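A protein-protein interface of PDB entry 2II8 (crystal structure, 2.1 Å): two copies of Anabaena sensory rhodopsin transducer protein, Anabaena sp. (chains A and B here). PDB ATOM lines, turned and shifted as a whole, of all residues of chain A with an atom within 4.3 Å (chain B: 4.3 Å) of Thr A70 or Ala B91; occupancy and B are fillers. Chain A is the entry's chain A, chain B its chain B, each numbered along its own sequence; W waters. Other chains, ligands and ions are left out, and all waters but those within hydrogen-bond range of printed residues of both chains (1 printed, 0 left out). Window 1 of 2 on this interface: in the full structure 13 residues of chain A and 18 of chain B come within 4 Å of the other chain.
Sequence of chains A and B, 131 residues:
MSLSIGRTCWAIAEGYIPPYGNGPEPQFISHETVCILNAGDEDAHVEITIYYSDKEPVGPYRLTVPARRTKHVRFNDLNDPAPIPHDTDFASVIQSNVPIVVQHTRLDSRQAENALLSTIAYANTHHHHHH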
ATOM      1  N   ILE A  36     -23.817  19.070 -15.050  1.00  0.00           N
ATOM      2  CA  ILE A  36     -24.997  19.855 -14.817  1.00  0.00           C
ATOM      3  C   ILE A  36     -24.814  20.627 -13.486  1.00  0.00           C
ATOM      4  O   ILE A  36     -24.321  20.026 -12.513  1.00  0.00           O
ATOM      5  CB  ILE A  36     -26.205  18.924 -14.663  1.00  0.00           C
ATOM      6  CG1 ILE A  36     -26.283  17.988 -15.875  1.00  0.00           C
ATOM      7  CG2 ILE A  36     -27.539  19.817 -14.551  1.00  0.00           C
ATOM      8  CD1 ILE A  36     -27.500  17.082 -15.891  1.00  0.00           C
ATOM      9  N   LEU A  37     -25.225  21.893 -13.450  1.00  0.00           N
ATOM     10  CA  LEU A  37     -25.289  22.690 -12.229  1.00  0.00           C
ATOM     11  C   LEU A  37     -26.703  23.101 -12.066  1.00  0.00           C
ATOM     12  O   LEU A  37     -27.313  23.666 -13.015  1.00  0.00           O
ATOM     13  CB  LEU A  37     -24.352  23.927 -12.338  1.00  0.00           C
ATOM     14  CG  LEU A  37     -24.643  25.065 -11.341  1.00  0.00           C
ATOM     15  CD1 LEU A  37     -24.179  24.604  -9.913  1.00  0.00           C
ATOM     16  CD2 LEU A  37     -23.865  26.294 -11.807  1.00  0.00           C
ATOM     17  N   VAL A  65     -31.068  16.435 -10.196  1.00  0.00           N
ATOM     18  CA  VAL A  65     -29.896  17.214  -9.727  1.00  0.00           C
ATOM     19  C   VAL A  65     -30.508  18.051  -8.576  1.00  0.00           C
ATOM     20  O   VAL A  65     -31.386  18.922  -8.837  1.00  0.00           O
ATOM     21  CB  VAL A  65     -29.252  18.103 -10.825  1.00  0.00           C
ATOM     22  CG1 VAL A  65     -28.010  18.795 -10.355  1.00  0.00           C
ATOM     23  CG2 VAL A  65     -28.962  17.242 -12.153  1.00  0.00           C
ATOM     24  N   ARG A  69     -26.778  22.143  -6.241  1.00  0.00           N
ATOM     25  CA  ARG A  69     -25.808  21.091  -6.432  1.00  0.00           C
ATOM     26  C   ARG A  69     -25.427  20.946  -7.885  1.00  0.00           C
ATOM     27  O   ARG A  69     -26.165  21.359  -8.800  1.00  0.00           O
ATOM     28  CB  ARG A  69     -26.326  19.722  -5.936  1.00  0.00           C
ATOM     29  CG  ARG A  69     -26.713  19.641  -4.418  1.00  0.00           C
ATOM     30  CD  ARG A  69     -25.500  19.842  -3.446  1.00  0.00           C
ATOM     31  NE  ARG A  69     -25.923  19.627  -2.070  1.00  0.00           N
ATOM     32  CZ  ARG A  69     -26.407  20.551  -1.230  1.00  0.00           C
ATOM     33  NH1 ARG A  69     -26.629  21.864  -1.565  1.00  0.00           N
ATOM     34  NH2 ARG A  69     -26.754  20.139   0.011  1.00  0.00           N
ATOM     35  N   THR A  70     -24.299  20.299  -8.085  1.00  0.00           N
ATOM     36  CA  THR A  70     -23.835  19.901  -9.384  1.00  0.00           C
ATOM     37  C   THR A  70     -23.909  18.339  -9.486  1.00  0.00           C
ATOM     38  O   THR A  70     -24.008  17.628  -8.473  1.00  0.00           O
ATOM     39  CB  THR A  70     -22.381  20.479  -9.601  1.00  0.00           C
ATOM     40  OG1 THR A  70     -22.022  20.342 -10.992  1.00  0.00           O
ATOM     41  CG2 THR A  70     -21.422  19.688  -8.726  1.00  0.00           C
ATOM     42  N   LYS A  71     -23.897  17.812 -10.703  1.00  0.00           N
ATOM     43  CA  LYS A  71     -23.856  16.390 -10.960  1.00  0.00           C
ATOM     44  C   LYS A  71     -23.196  16.174 -12.277  1.00  0.00           C
ATOM     45  O   LYS A  71     -23.503  16.867 -13.221  1.00  0.00           O
ATOM     46  CB  LYS A  71     -25.256  15.805 -10.990  1.00  0.00           C
ATOM     47  CG  LYS A  71     -25.337  14.269 -10.919  1.00  0.00           C
ATOM     48  CD  LYS A  71     -26.752  13.899 -10.574  1.00  0.00           C
ATOM     49  CE  LYS A  71     -26.852  12.613  -9.774  1.00  0.00           C
ATOM     50  NZ  LYS A  71     -28.228  12.426  -9.183  1.00  0.00           N
ATOM     51  N   HIS A  72     -22.317  15.178 -12.349  1.00  0.00           N
ATOM     52  CA  HIS A  72     -21.621  14.811 -13.590  1.00  0.00           C
ATOM     53  C   HIS A  72     -22.268  13.522 -14.044  1.00  0.00           C
ATOM     54  O   HIS A  72     -22.444  12.582 -13.266  1.00  0.00           O
ATOM     55  CB  HIS A  72     -20.104  14.668 -13.387  1.00  0.00           C
ATOM     56  CG  HIS A  72     -19.420  15.969 -13.106  1.00  0.00           C
ATOM     57  ND1 HIS A  72     -18.086  16.183 -13.373  1.00  0.00           N
ATOM     58  CD2 HIS A  72     -19.892  17.129 -12.598  1.00  0.00           C
ATOM     59  CE1 HIS A  72     -17.760  17.416 -13.019  1.00  0.00           C
ATOM     60  NE2 HIS A  72     -18.840  18.020 -12.554  1.00  0.00           N
ATOM     61  N   ILE B  12     -20.238  28.207 -14.785  1.00  0.00           N
ATOM     62  CA  ILE B  12     -19.364  27.231 -15.393  1.00  0.00           C
ATOM     63  C   ILE B  12     -19.725  25.887 -14.755  1.00  0.00           C
ATOM     64  O   ILE B  12     -19.450  25.685 -13.569  1.00  0.00           O
ATOM     65  CB  ILE B  12     -17.906  27.593 -15.131  1.00  0.00           C
ATOM     66  CG1 ILE B  12     -17.624  28.981 -15.697  1.00  0.00           C
ATOM     67  CG2 ILE B  12     -16.906  26.553 -15.789  1.00  0.00           C
ATOM     68  CD1 ILE B  12     -16.248  29.473 -15.569  1.00  0.00           C
ATOM     69  N   ALA B  13     -20.287  24.949 -15.543  1.00  0.00           N
ATOM     70  CA  ALA B  13     -20.786  23.680 -14.994  1.00  0.00           C
ATOM     71  C   ALA B  13     -19.730  22.645 -14.641  1.00  0.00           C
ATOM     72  O   ALA B  13     -19.999  21.717 -13.911  1.00  0.00           O
ATOM     73  CB  ALA B  13     -21.836  23.091 -15.856  1.00  0.00           C
ATOM     74  N   THR B  49     -19.101  31.724  -6.428  1.00  0.00           N
ATOM     75  CA  THR B  49     -19.667  30.680  -5.600  1.00  0.00           C
ATOM     76  C   THR B  49     -19.281  29.339  -6.195  1.00  0.00           C
ATOM     77  O   THR B  49     -19.378  29.161  -7.448  1.00  0.00           O
ATOM     78  CB  THR B  49     -21.170  30.790  -5.568  1.00  0.00           C
ATOM     79  OG1 THR B  49     -21.515  32.090  -5.152  1.00  0.00           O
ATOM     80  CG2 THR B  49     -21.822  29.783  -4.608  1.00  0.00           C
ATOM     81  N   ILE B  50     -18.891  28.381  -5.331  1.00  0.00           N
ATOM     82  CA  ILE B  50     -18.455  27.100  -5.772  1.00  0.00           C
ATOM     83  C   ILE B  50     -19.506  26.110  -5.328  1.00  0.00           C
ATOM     84  O   ILE B  50     -19.926  26.145  -4.138  1.00  0.00           O
ATOM     85  CB  ILE B  50     -17.037  26.737  -5.217  1.00  0.00           C
ATOM     86  CG1 ILE B  50     -15.990  27.791  -5.616  1.00  0.00           C
ATOM     87  CG2 ILE B  50     -16.595  25.307  -5.653  1.00  0.00           C
ATOM     88  CD1 ILE B  50     -15.686  27.801  -7.104  1.00  0.00           C
ATOM     89  N   TYR B  51     -19.940  25.247  -6.278  1.00  0.00           N
ATOM     90  CA  TYR B  51     -20.994  24.262  -6.058  1.00  0.00           C
ATOM     91  C   TYR B  51     -20.388  22.879  -6.100  1.00  0.00           C
ATOM     92  O   TYR B  51     -19.465  22.627  -6.842  1.00  0.00           O
ATOM     93  CB  TYR B  51     -22.174  24.388  -7.086  1.00  0.00           C
ATOM     94  CG  TYR B  51     -22.971  25.683  -6.933  1.00  0.00           C
ATOM     95  CD1 TYR B  51     -22.466  26.930  -7.442  1.00  0.00           C
ATOM     96  CD2 TYR B  51     -24.185  25.678  -6.304  1.00  0.00           C
ATOM     97  CE1 TYR B  51     -23.232  28.146  -7.260  1.00  0.00           C
ATOM     98  CE2 TYR B  51     -24.947  26.862  -6.138  1.00  0.00           C
ATOM     99  CZ  TYR B  51     -24.425  28.078  -6.622  1.00  0.00           C
ATOM    100  OH  TYR B  51     -25.155  29.207  -6.453  1.00  0.00           O
ATOM    101  N   TYR B  52     -20.977  21.967  -5.324  1.00  0.00           N
ATOM    102  CA  TYR B  52     -20.512  20.605  -5.238  1.00  0.00           C
ATOM    103  C   TYR B  52     -21.682  19.633  -5.455  1.00  0.00           C
ATOM    104  O   TYR B  52     -22.831  20.073  -5.506  1.00  0.00           O
ATOM    105  CB  TYR B  52     -19.868  20.382  -3.840  1.00  0.00           C
ATOM    106  CG  TYR B  52     -18.639  21.210  -3.627  1.00  0.00           C
ATOM    107  CD1 TYR B  52     -17.418  20.793  -4.126  1.00  0.00           C
ATOM    108  CD2 TYR B  52     -18.710  22.427  -2.917  1.00  0.00           C
ATOM    109  CE1 TYR B  52     -16.301  21.547  -3.965  1.00  0.00           C
ATOM    110  CE2 TYR B  52     -17.591  23.191  -2.699  1.00  0.00           C
ATOM    111  CZ  TYR B  52     -16.383  22.765  -3.252  1.00  0.00           C
ATOM    112  OH  TYR B  52     -15.247  23.527  -3.126  1.00  0.00           O
ATOM    113  N   SER B  53     -21.369  18.335  -5.619  1.00  0.00           N
ATOM    114  CA  SER B  53     -22.404  17.286  -5.828  1.00  0.00           C
ATOM    115  C   SER B  53     -23.092  16.881  -4.538  1.00  0.00           C
ATOM    116  O   SER B  53     -24.256  16.374  -4.533  1.00  0.00           O
ATOM    117  CB  SER B  53     -21.834  16.036  -6.499  1.00  0.00           C
ATOM    118  OG  SER B  53     -20.850  15.458  -5.635  1.00  0.00           O
ATOM    119  N   PHE B  90     -16.657  20.120  -9.157  1.00  0.00           N
ATOM    120  CA  PHE B  90     -17.402  21.295  -8.692  1.00  0.00           C
ATOM    121  C   PHE B  90     -17.892  22.091  -9.937  1.00  0.00           C
ATOM    122  O   PHE B  90     -17.553  21.726 -11.092  1.00  0.00           O
ATOM    123  CB  PHE B  90     -16.540  22.153  -7.740  1.00  0.00           C
ATOM    124  CG  PHE B  90     -15.319  22.736  -8.377  1.00  0.00           C
ATOM    125  CD1 PHE B  90     -14.110  22.014  -8.415  1.00  0.00           C
ATOM    126  CD2 PHE B  90     -15.341  24.018  -8.936  1.00  0.00           C
ATOM    127  CE1 PHE B  90     -12.968  22.574  -9.030  1.00  0.00           C
ATOM    128  CE2 PHE B  90     -14.200  24.552  -9.575  1.00  0.00           C
ATOM    129  CZ  PHE B  90     -13.030  23.844  -9.630  1.00  0.00           C
ATOM    130  N   ALA B  91     -18.618  23.170  -9.662  1.00  0.00           N
ATOM    131  CA  ALA B  91     -19.162  24.090 -10.679  1.00  0.00           C
ATOM    132  C   ALA B  91     -19.052  25.467 -10.033  1.00  0.00           C
ATOM    133  O   ALA B  91     -18.850  25.580  -8.798  1.00  0.00           O
ATOM    134  CB  ALA B  91     -20.618  23.696 -10.998  1.00  0.00           C
ATOM    135  N   SER B  92     -19.069  26.540 -10.822  1.00  0.00           N
ATOM    136  CA  SER B  92     -19.082  27.903 -10.207  1.00  0.00           C
ATOM    137  C   SER B  92     -20.048  28.877 -10.860  1.00  0.00           C
ATOM    138  O   SER B  92     -20.410  28.717 -12.033  1.00  0.00           O
ATOM    139  CB  SER B  92     -17.707  28.486 -10.305  1.00  0.00           C
ATOM    140  OG  SER B  92     -17.291  28.462 -11.660  1.00  0.00           O
HETATM  141  O   HOH W   1     -25.818  15.747  -6.753  1.00  0.00           O
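The backbone carbonyl oxygen of Tyr B52 lies within hydrogen-bond range of the backbone NH of Thr A70 (3.0 Å).
No position is printed for both chains.
Of the 7 printed residues of chain A, 3 touch a printed residue of chain B. Printed residues of chain A that touch a printed residue of chain B: Leu A37, Arg A69 and Thr A70. Printed residues of chain B that touch a printed residue of chain A: Ala B13, Tyr B51, Tyr B52, Ser B53 and Ala B91. Among the printed residues, 8 pairs touch across the chains.
Among the printed residues, pairs that only touch across the chains: Leu A37 with Tyr B51 (3.4 Å), Leu A37 with Ala B91 (3.8 Å), Arg A69 with Tyr B52 (3.3 Å), Arg A69 with Ser B53 (3.8 Å), Thr A70 with Ala B13 (3.8 Å), Thr A70 with Ser B53 (3.1 Å) and Thr A70 with Ala B91 (3.6 Å).
Of the printed residues of chain B, Leu A37 touches Tyr B51 and Ala B91. Of the printed residues of chain B, Thr A70 touches Ala B13 (3.8 Å), Tyr B52 (3.0 Å), Ser B53 (3.1 Å) and Ala B91 (3.6 Å). Of the printed residues of chain A, Ala B13 touches Thr A70. Of the printed residues of chain A, Tyr B51 touches Leu A37 (3.4 Å). Of the printed residues of chain A, Tyr B52 touches Arg A69 and Thr A70. Of the printed residues of chain A, Ser B53 touches Arg A69 and Thr A70. Ala B91 touches just these residues of chain A: Leu A37 (3.8 Å) and Thr A70 (3.6 Å). Ser B92 touches none of the printed residues of chain A. The nearest printed residue of chain B that does not touch Thr A70 is Tyr B51 (4.002 Å). The nearest printed residue of chain A that does not touch Ala B91 is Ile A36 (5.4 Å). The nearest printed residue of chain B that does not touch Arg A69 is Tyr B51 (4.4 Å).
Water W1 lies within hydrogen-bond range of O of Ser B53 (2.8 Å) and O of Thr A70 (3.1 Å).
The backbone carbonyl oxygen (O) of Ile A36 lies within hydrogen-bond range of the side-chain hydroxyl (OG1) of Thr A70, at 2.8 Å. The backbone NH (N) of Tyr B51 lies within hydrogen-bond range of the backbone carbonyl oxygen (O) of Ala B91 (2.8 Å).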
